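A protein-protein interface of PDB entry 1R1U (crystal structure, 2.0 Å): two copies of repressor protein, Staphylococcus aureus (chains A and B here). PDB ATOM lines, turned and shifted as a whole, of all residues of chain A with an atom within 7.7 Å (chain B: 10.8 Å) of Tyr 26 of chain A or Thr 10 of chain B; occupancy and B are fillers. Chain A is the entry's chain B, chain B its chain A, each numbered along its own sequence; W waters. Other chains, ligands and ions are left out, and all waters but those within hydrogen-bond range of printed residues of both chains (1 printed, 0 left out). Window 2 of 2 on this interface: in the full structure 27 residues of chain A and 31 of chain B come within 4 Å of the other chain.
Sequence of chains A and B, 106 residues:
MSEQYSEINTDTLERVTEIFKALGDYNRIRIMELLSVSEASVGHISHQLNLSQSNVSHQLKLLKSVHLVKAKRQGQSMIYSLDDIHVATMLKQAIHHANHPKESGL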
ATOM      1  N   ALA A  22     -19.835 -28.034  14.740  1.00  0.00           N
ATOM      2  CA  ALA A  22     -19.761 -26.694  14.146  1.00  0.00           C
ATOM      3  C   ALA A  22     -20.892 -25.773  14.477  1.00  0.00           C
ATOM      4  O   ALA A  22     -20.710 -24.539  14.507  1.00  0.00           O
ATOM      5  CB  ALA A  22     -19.662 -26.764  12.687  1.00  0.00           C
ATOM      6  N   LEU A  23     -22.068 -26.316  14.729  1.00  0.00           N
ATOM      7  CA  LEU A  23     -23.199 -25.486  15.046  1.00  0.00           C
ATOM      8  C   LEU A  23     -23.282 -25.203  16.547  1.00  0.00           C
ATOM      9  O   LEU A  23     -24.021 -24.358  16.988  1.00  0.00           O
ATOM     10  CB  LEU A  23     -24.465 -26.142  14.539  1.00  0.00           C
ATOM     11  CG  LEU A  23     -24.608 -26.108  13.007  1.00  0.00           C
ATOM     12  CD1 LEU A  23     -25.621 -27.124  12.426  1.00  0.00           C
ATOM     13  CD2 LEU A  23     -24.875 -24.735  12.493  1.00  0.00           C
ATOM     14  N   GLY A  24     -22.506 -25.933  17.341  1.00  0.00           N
ATOM     15  CA  GLY A  24     -22.539 -25.741  18.772  1.00  0.00           C
ATOM     16  C   GLY A  24     -21.862 -24.463  19.285  1.00  0.00           C
ATOM     17  O   GLY A  24     -21.015 -24.561  20.183  1.00  0.00           O
ATOM     18  N   ASP A  25     -22.295 -23.271  18.830  1.00  0.00           N
ATOM     19  CA  ASP A  25     -21.587 -22.061  19.196  1.00  0.00           C
ATOM     20  C   ASP A  25     -22.474 -20.866  18.927  1.00  0.00           C
ATOM     21  O   ASP A  25     -23.069 -20.735  17.835  1.00  0.00           O
ATOM     22  CB  ASP A  25     -20.309 -21.948  18.393  1.00  0.00           C
ATOM     23  CG  ASP A  25     -19.588 -20.659  18.664  1.00  0.00           C
ATOM     24  OD1 ASP A  25     -19.800 -19.640  17.910  1.00  0.00           O
ATOM     25  OD2 ASP A  25     -18.757 -20.588  19.601  1.00  0.00           O
ATOM     26  N   TYR A  26     -22.643 -20.045  19.956  1.00  0.00           N
ATOM     27  CA  TYR A  26     -23.490 -18.877  19.885  1.00  0.00           C
ATOM     28  C   TYR A  26     -23.275 -17.975  18.666  1.00  0.00           C
ATOM     29  O   TYR A  26     -24.253 -17.645  17.946  1.00  0.00           O
ATOM     30  CB  TYR A  26     -23.303 -18.097  21.159  1.00  0.00           C
ATOM     31  CG  TYR A  26     -24.220 -16.903  21.318  1.00  0.00           C
ATOM     32  CD1 TYR A  26     -25.497 -17.054  21.848  1.00  0.00           C
ATOM     33  CD2 TYR A  26     -23.769 -15.627  21.057  1.00  0.00           C
ATOM     34  CE1 TYR A  26     -26.313 -15.957  22.044  1.00  0.00           C
ATOM     35  CE2 TYR A  26     -24.574 -14.515  21.300  1.00  0.00           C
ATOM     36  CZ  TYR A  26     -25.841 -14.703  21.768  1.00  0.00           C
ATOM     37  OH  TYR A  26     -26.650 -13.630  21.976  1.00  0.00           O
ATOM     38  N   ASN A  27     -22.028 -17.606  18.399  1.00  0.00           N
ATOM     39  CA  ASN A  27     -21.749 -16.742  17.261  1.00  0.00           C
ATOM     40  C   ASN A  27     -21.874 -17.411  15.909  1.00  0.00           C
ATOM     41  O   ASN A  27     -22.315 -16.736  14.945  1.00  0.00           O
ATOM     42  CB  ASN A  27     -20.432 -15.994  17.391  1.00  0.00           C
ATOM     43  CG  ASN A  27     -20.500 -14.884  18.442  1.00  0.00           C
ATOM     44  OD1 ASN A  27     -21.566 -14.305  18.695  1.00  0.00           O
ATOM     45  ND2 ASN A  27     -19.373 -14.610  19.086  1.00  0.00           N
ATOM     46  N   ARG A  28     -21.586 -18.708  15.805  1.00  0.00           N
ATOM     47  CA  ARG A  28     -21.817 -19.403  14.524  1.00  0.00           C
ATOM     48  C   ARG A  28     -23.313 -19.554  14.202  1.00  0.00           C
ATOM     49  O   ARG A  28     -23.713 -19.430  13.039  1.00  0.00           O
ATOM     50  CB  ARG A  28     -21.058 -20.733  14.422  1.00  0.00           C
ATOM     51  CG  ARG A  28     -19.535 -20.527  14.314  1.00  0.00           C
ATOM     52  CD  ARG A  28     -18.767 -21.742  13.964  1.00  0.00           C
ATOM     53  NE  ARG A  28     -18.690 -22.766  14.971  1.00  0.00           N
ATOM     54  CZ  ARG A  28     -17.817 -22.825  16.006  1.00  0.00           C
ATOM     55  NH1 ARG A  28     -16.923 -21.872  16.276  1.00  0.00           N
ATOM     56  NH2 ARG A  28     -17.851 -23.878  16.797  1.00  0.00           N
ATOM     57  N   ILE A  29     -24.134 -19.681  15.241  1.00  0.00           N
ATOM     58  CA  ILE A  29     -25.573 -19.740  15.120  1.00  0.00           C
ATOM     59  C   ILE A  29     -26.146 -18.404  14.694  1.00  0.00           C
ATOM     60  O   ILE A  29     -27.001 -18.366  13.759  1.00  0.00           O
ATOM     61  CB  ILE A  29     -26.219 -20.191  16.382  1.00  0.00           C
ATOM     62  CG1 ILE A  29     -25.744 -21.579  16.698  1.00  0.00           C
ATOM     63  CG2 ILE A  29     -27.798 -20.099  16.267  1.00  0.00           C
ATOM     64  CD1 ILE A  29     -26.539 -22.569  16.122  1.00  0.00           C
ATOM     65  N   ARG A  30     -25.627 -17.318  15.275  1.00  0.00           N
ATOM     66  CA  ARG A  30     -25.993 -15.975  14.822  1.00  0.00           C
ATOM     67  C   ARG A  30     -25.667 -15.760  13.338  1.00  0.00           C
ATOM     68  O   ARG A  30     -26.523 -15.248  12.594  1.00  0.00           O
ATOM     69  CB  ARG A  30     -25.366 -14.868  15.646  1.00  0.00           C
ATOM     70  CG  ARG A  30     -25.759 -14.862  17.116  1.00  0.00           C
ATOM     71  CD  ARG A  30     -25.944 -13.428  17.689  1.00  0.00           C
ATOM     72  NE  ARG A  30     -24.651 -12.937  17.791  1.00  0.00           N
ATOM     73  CZ  ARG A  30     -24.206 -11.727  17.606  1.00  0.00           C
ATOM     74  NH1 ARG A  30     -24.948 -10.687  17.301  1.00  0.00           N
ATOM     75  NH2 ARG A  30     -22.924 -11.616  17.788  1.00  0.00           N
ATOM     76  N   ILE A  31     -24.490 -16.173  12.898  1.00  0.00           N
ATOM     77  CA  ILE A  31     -24.115 -16.110  11.458  1.00  0.00           C
ATOM     78  C   ILE A  31     -25.006 -16.995  10.549  1.00  0.00           C
ATOM     79  O   ILE A  31     -25.414 -16.574   9.463  1.00  0.00           O
ATOM     80  CB  ILE A  31     -22.687 -16.533  11.272  1.00  0.00           C
ATOM     81  CG1 ILE A  31     -21.740 -15.569  11.914  1.00  0.00           C
ATOM     82  CG2 ILE A  31     -22.272 -16.657   9.795  1.00  0.00           C
ATOM     83  CD1 ILE A  31     -20.266 -16.088  11.914  1.00  0.00           C
ATOM     84  N   MET A  32     -25.261 -18.220  10.959  1.00  0.00           N
ATOM     85  CA  MET A  32     -26.225 -19.061  10.250  1.00  0.00           C
ATOM     86  C   MET A  32     -27.621 -18.483  10.121  1.00  0.00           C
ATOM     87  O   MET A  32     -28.235 -18.598   9.031  1.00  0.00           O
ATOM     88  CB  MET A  32     -26.310 -20.443  10.863  1.00  0.00           C
ATOM     89  CG  MET A  32     -25.039 -21.243  10.774  1.00  0.00           C
ATOM     90  SD  MET A  32     -24.528 -21.820   9.125  1.00  0.00           S
ATOM     91  CE  MET A  32     -25.815 -23.158   8.891  1.00  0.00           C
ATOM     92  N   LEU A  49     -23.942  -8.218  13.126  1.00  0.00           N
ATOM     93  CA  LEU A  49     -23.709  -8.984  14.347  1.00  0.00           C
ATOM     94  C   LEU A  49     -22.675  -8.394  15.296  1.00  0.00           C
ATOM     95  O   LEU A  49     -22.383  -9.024  16.339  1.00  0.00           O
ATOM     96  CB  LEU A  49     -23.248 -10.375  13.966  1.00  0.00           C
ATOM     97  CG  LEU A  49     -24.253 -11.084  13.017  1.00  0.00           C
ATOM     98  CD1 LEU A  49     -23.761 -12.481  12.706  1.00  0.00           C
ATOM     99  CD2 LEU A  49     -25.594 -11.191  13.641  1.00  0.00           C
ATOM    100  N   LEU A  51     -19.437  -8.244  15.007  1.00  0.00           N
ATOM    101  CA  LEU A  51     -18.313  -9.155  15.042  1.00  0.00           C
ATOM    102  C   LEU A  51     -17.285  -8.630  14.082  1.00  0.00           C
ATOM    103  O   LEU A  51     -17.637  -8.130  13.025  1.00  0.00           O
ATOM    104  CB  LEU A  51     -18.761 -10.558  14.591  1.00  0.00           C
ATOM    105  CG  LEU A  51     -19.794 -11.255  15.439  1.00  0.00           C
ATOM    106  CD1 LEU A  51     -20.192 -12.598  14.777  1.00  0.00           C
ATOM    107  CD2 LEU A  51     -19.251 -11.493  16.876  1.00  0.00           C
ATOM    108  N   ASN B   9     -33.973 -13.590  18.581  1.00  0.00           N
ATOM    109  CA  ASN B   9     -33.615 -12.949  19.881  1.00  0.00           C
ATOM    110  C   ASN B   9     -32.572 -13.751  20.699  1.00  0.00           C
ATOM    111  O   ASN B   9     -32.161 -14.833  20.284  1.00  0.00           O
ATOM    112  CB  ASN B   9     -34.882 -12.671  20.718  1.00  0.00           C
ATOM    113  CG  ASN B   9     -35.427 -13.911  21.402  1.00  0.00           C
ATOM    114  OD1 ASN B   9     -35.146 -14.174  22.578  1.00  0.00           O
ATOM    115  ND2 ASN B   9     -36.237 -14.670  20.673  1.00  0.00           N
ATOM    116  N   THR B  10     -32.178 -13.206  21.863  1.00  0.00           N
ATOM    117  CA  THR B  10     -31.040 -13.705  22.672  1.00  0.00           C
ATOM    118  C   THR B  10     -31.269 -15.076  23.305  1.00  0.00           C
ATOM    119  O   THR B  10     -30.399 -15.946  23.239  1.00  0.00           O
ATOM    120  CB  THR B  10     -30.690 -12.660  23.792  1.00  0.00           C
ATOM    121  OG1 THR B  10     -29.741 -11.716  23.287  1.00  0.00           O
ATOM    122  CG2 THR B  10     -29.986 -13.280  25.004  1.00  0.00           C
ATOM    123  N   ASP B  11     -32.420 -15.240  23.950  1.00  0.00           N
ATOM    124  CA  ASP B  11     -32.716 -16.442  24.715  1.00  0.00           C
ATOM    125  C   ASP B  11     -33.132 -17.608  23.846  1.00  0.00           C
ATOM    126  O   ASP B  11     -32.815 -18.738  24.162  1.00  0.00           O
ATOM    127  CB  ASP B  11     -33.755 -16.123  25.779  1.00  0.00           C
ATOM    128  CG  ASP B  11     -33.273 -14.995  26.684  1.00  0.00           C
ATOM    129  OD1 ASP B  11     -32.550 -15.292  27.673  1.00  0.00           O
ATOM    130  OD2 ASP B  11     -33.474 -13.782  26.416  1.00  0.00           O
ATOM    131  N   THR B  12     -33.809 -17.312  22.741  1.00  0.00           N
ATOM    132  CA  THR B  12     -34.006 -18.276  21.678  1.00  0.00           C
ATOM    133  C   THR B  12     -32.637 -18.785  21.194  1.00  0.00           C
ATOM    134  O   THR B  12     -32.430 -19.966  21.074  1.00  0.00           O
ATOM    135  CB  THR B  12     -34.796 -17.650  20.493  1.00  0.00           C
ATOM    136  OG1 THR B  12     -36.153 -17.406  20.895  1.00  0.00           O
ATOM    137  CG2 THR B  12     -34.905 -18.629  19.302  1.00  0.00           C
ATOM    138  N   LEU B  13     -31.706 -17.887  20.933  1.00  0.00           N
ATOM    139  CA  LEU B  13     -30.431 -18.306  20.347  1.00  0.00           C
ATOM    140  C   LEU B  13     -29.543 -19.075  21.353  1.00  0.00           C
ATOM    141  O   LEU B  13     -28.735 -19.875  20.908  1.00  0.00           O
ATOM    142  CB  LEU B  13     -29.682 -17.135  19.696  1.00  0.00           C
ATOM    143  CG  LEU B  13     -30.335 -16.599  18.410  1.00  0.00           C
ATOM    144  CD1 LEU B  13     -29.582 -15.417  17.800  1.00  0.00           C
ATOM    145  CD2 LEU B  13     -30.554 -17.701  17.336  1.00  0.00           C
ATOM    146  N   GLU B  14     -29.741 -18.867  22.667  1.00  0.00           N
ATOM    147  CA  GLU B  14     -29.041 -19.639  23.700  1.00  0.00           C
ATOM    148  C   GLU B  14     -29.623 -21.051  23.810  1.00  0.00           C
ATOM    149  O   GLU B  14     -28.889 -22.035  23.896  1.00  0.00           O
ATOM    150  CB  GLU B  14     -29.046 -18.932  25.056  1.00  0.00           C
ATOM    151  CG  GLU B  14     -28.279 -17.599  25.072  1.00  0.00           C
ATOM    152  CD  GLU B  14     -26.772 -17.709  25.420  1.00  0.00           C
ATOM    153  OE1 GLU B  14     -26.343 -16.822  26.203  1.00  0.00           O
ATOM    154  OE2 GLU B  14     -26.015 -18.646  24.920  1.00  0.00           O
ATOM    155  N   ARG B  15     -30.930 -21.160  23.724  1.00  0.00           N
ATOM    156  CA  ARG B  15     -31.541 -22.474  23.692  1.00  0.00           C
ATOM    157  C   ARG B  15     -31.077 -23.246  22.474  1.00  0.00           C
ATOM    158  O   ARG B  15     -30.707 -24.396  22.632  1.00  0.00           O
ATOM    159  CB  ARG B  15     -33.068 -22.396  23.751  1.00  0.00           C
ATOM    160  CG  ARG B  15     -33.616 -22.238  25.178  1.00  0.00           C
ATOM    161  CD  ARG B  15     -35.147 -22.394  25.280  1.00  0.00           C
ATOM    162  NE  ARG B  15     -35.790 -21.303  24.541  1.00  0.00           N
ATOM    163  CZ  ARG B  15     -36.352 -20.214  25.088  1.00  0.00           C
ATOM    164  NH1 ARG B  15     -36.372 -20.034  26.413  1.00  0.00           N
ATOM    165  NH2 ARG B  15     -36.903 -19.283  24.296  1.00  0.00           N
ATOM    166  N   VAL B  16     -31.027 -22.635  21.286  1.00  0.00           N
ATOM    167  CA  VAL B  16     -30.569 -23.393  20.112  1.00  0.00           C
ATOM    168  C   VAL B  16     -29.093 -23.706  20.112  1.00  0.00           C
ATOM    169  O   VAL B  16     -28.678 -24.729  19.568  1.00  0.00           O
ATOM    170  CB  VAL B  16     -31.030 -22.880  18.696  1.00  0.00           C
ATOM    171  CG1 VAL B  16     -32.016 -21.761  18.757  1.00  0.00           C
ATOM    172  CG2 VAL B  16     -29.896 -22.586  17.780  1.00  0.00           C
ATOM    173  N   THR B  17     -28.313 -22.832  20.727  1.00  0.00           N
ATOM    174  CA  THR B  17     -26.915 -23.113  21.005  1.00  0.00           C
ATOM    175  C   THR B  17     -26.774 -24.357  21.886  1.00  0.00           C
ATOM    176  O   THR B  17     -25.942 -25.189  21.623  1.00  0.00           O
ATOM    177  CB  THR B  17     -26.288 -21.893  21.682  1.00  0.00           C
ATOM    178  OG1 THR B  17     -26.220 -20.814  20.737  1.00  0.00           O
ATOM    179  CG2 THR B  17     -24.829 -22.187  22.055  1.00  0.00           C
ATOM    180  N   GLU B  18     -27.609 -24.463  22.901  1.00  0.00           N
ATOM    181  CA  GLU B  18     -27.667 -25.621  23.815  1.00  0.00           C
ATOM    182  C   GLU B  18     -28.061 -26.897  23.066  1.00  0.00           C
ATOM    183  O   GLU B  18     -27.522 -27.986  23.315  1.00  0.00           O
ATOM    184  CB  GLU B  18     -28.678 -25.369  24.893  1.00  0.00           C
ATOM    185  CG  GLU B  18     -28.161 -25.580  26.286  1.00  0.00           C
ATOM    186  CD  GLU B  18     -27.304 -24.448  26.753  1.00  0.00           C
ATOM    187  OE1 GLU B  18     -26.428 -24.012  25.970  1.00  0.00           O
ATOM    188  OE2 GLU B  18     -27.502 -23.983  27.902  1.00  0.00           O
ATOM    189  N   ILE B  19     -29.014 -26.748  22.142  1.00  0.00           N
ATOM    190  CA  ILE B  19     -29.512 -27.860  21.327  1.00  0.00           C
ATOM    191  C   ILE B  19     -28.409 -28.421  20.492  1.00  0.00           C
ATOM    192  O   ILE B  19     -28.208 -29.621  20.439  1.00  0.00           O
ATOM    193  CB  ILE B  19     -30.740 -27.422  20.471  1.00  0.00           C
ATOM    194  CG1 ILE B  19     -32.000 -27.463  21.369  1.00  0.00           C
ATOM    195  CG2 ILE B  19     -30.889 -28.285  19.235  1.00  0.00           C
ATOM    196  CD1 ILE B  19     -33.122 -26.645  20.843  1.00  0.00           C
ATOM    197  N   PHE B  20     -27.671 -27.549  19.845  1.00  0.00           N
ATOM    198  CA  PHE B  20     -26.632 -27.981  18.971  1.00  0.00           C
ATOM    199  C   PHE B  20     -25.390 -28.538  19.693  1.00  0.00           C
ATOM    200  O   PHE B  20     -24.782 -29.494  19.196  1.00  0.00           O
ATOM    201  CB  PHE B  20     -26.320 -26.903  17.980  1.00  0.00           C
ATOM    202  CG  PHE B  20     -27.409 -26.733  16.868  1.00  0.00           C
ATOM    203  CD1 PHE B  20     -28.034 -27.806  16.294  1.00  0.00           C
ATOM    204  CD2 PHE B  20     -27.731 -25.473  16.388  1.00  0.00           C
ATOM    205  CE1 PHE B  20     -28.988 -27.621  15.295  1.00  0.00           C
ATOM    206  CE2 PHE B  20     -28.667 -25.299  15.391  1.00  0.00           C
ATOM    207  CZ  PHE B  20     -29.310 -26.376  14.866  1.00  0.00           C
ATOM    208  N   LYS B  21     -25.072 -27.997  20.878  1.00  0.00           N
ATOM    209  CA  LYS B  21     -23.960 -28.550  21.752  1.00  0.00           C
ATOM    210  C   LYS B  21     -24.283 -30.002  22.136  1.00  0.00           C
ATOM    211  O   LYS B  21     -23.464 -30.912  21.947  1.00  0.00           O
ATOM    212  CB  LYS B  21     -23.782 -27.648  22.974  1.00  0.00           C
ATOM    213  CG  LYS B  21     -23.080 -26.320  22.657  1.00  0.00           C
ATOM    214  CD  LYS B  21     -22.739 -25.412  23.931  1.00  0.00           C
ATOM    215  CE  LYS B  21     -21.850 -24.206  23.444  1.00  0.00           C
ATOM    216  NZ  LYS B  21     -21.635 -23.108  24.377  1.00  0.00           N
HETATM  217  O   HOH W   1     -21.221 -20.648  22.698  1.00  0.00           O
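Water W1 lies within hydrogen-bond range of the side-chain amino group of Lys 21 of chain B and the backbone NH of Tyr 26 of chain A.
Phe 20 of chain B touches Leu 23 of chain A (CB to O, 3.6 Å).
Gly 24 of chain A touches Phe 20 of chain B.
Gly 24 of chain A touches Lys 21 of chain B (O to CE, 3.4 Å).
Thr 10 of chain B touches Tyr 26 of chain A.
Tyr 26 of chain A touches Glu 14 of chain B.
OG1 of Thr 17 of chain B touches CA of Tyr 26 of chain A (3.5 Å).
CD2 of Leu 13 of chain B touches CG2 of Ile 29 of chain A, at 3.8 Å.
Ile 29 of chain A touches Val 16 of chain B (CG2 to CG2, 3.6 Å).
Phe 20 of chain B touches Ile 29 of chain A (CD2 to CD1, 3.2 Å).
Arg 30 of chain A touches Leu 13 of chain B.
Of the 13 printed residues of chain B, 7 touch a printed residue of chain A.
Hydrophobic or aromatic side chains of chain B that line the printed part of chain A: Leu 13, Val 16 and Phe 20.
Of the 13 printed residues of chain A, 5 touch a printed residue of chain B.
O of Leu 49 of chain A lies within hydrogen-bond range of NH2 of Arg 30 of chain A, at 3.0 Å.
NH2 of Arg 30 of chain A is in hydrogen-bond range of OD1 of Asn 27 of chain A (3.1 Å).
The side-chain hydroxyl (OG1) of Thr 17 of chain B lies within hydrogen-bond range of the backbone carbonyl oxygen (O) of Leu 13 of chain B, 2.7 Å away.
Printed residues of chain B within 4 Å of Leu 23 of chain A: Phe 20.
No residue of chain B comes within 4 Å of Asp 25 of chain A.
Of the printed residues of chain B, Tyr 26 of chain A touches Thr 10, Glu 14 and Thr 17.
Asn 27 of chain A touches none of the printed residues of chain B.
Arg 28 of chain A touches none of the printed residues of chain B.
Of chain B, only Leu 13 comes within 4 Å of Arg 30 of chain A.
Of the printed residues of chain A, Thr 10 of chain B touches Tyr 26 (3.9 Å).
Printed residues of chain A within 4 Å of Leu 13 of chain B: Ile 29 (3.8 Å) and Arg 30 (3.9 Å).
Printed residues of chain A within 4 Å of Val 16 of chain B: Ile 29 (3.6 Å).
Printed residues of chain A within 4 Å of Thr 17 of chain B: Tyr 26 (3.5 Å).
Of the printed residues of chain A, Lys 21 of chain B touches Gly 24.
The nearest residue of chain B that does not touch Tyr 26 of chain A is Leu 13 of chain B (4.3 Å).
The nearest printed residue of chain B that does not touch Gly 24 of chain A is Thr 17 of chain B (4.5 Å).
No position is printed for both chains.
Of the 10 pairs that touch across the chains among the printed residues, none has its exchanged pair printed and touching as well.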
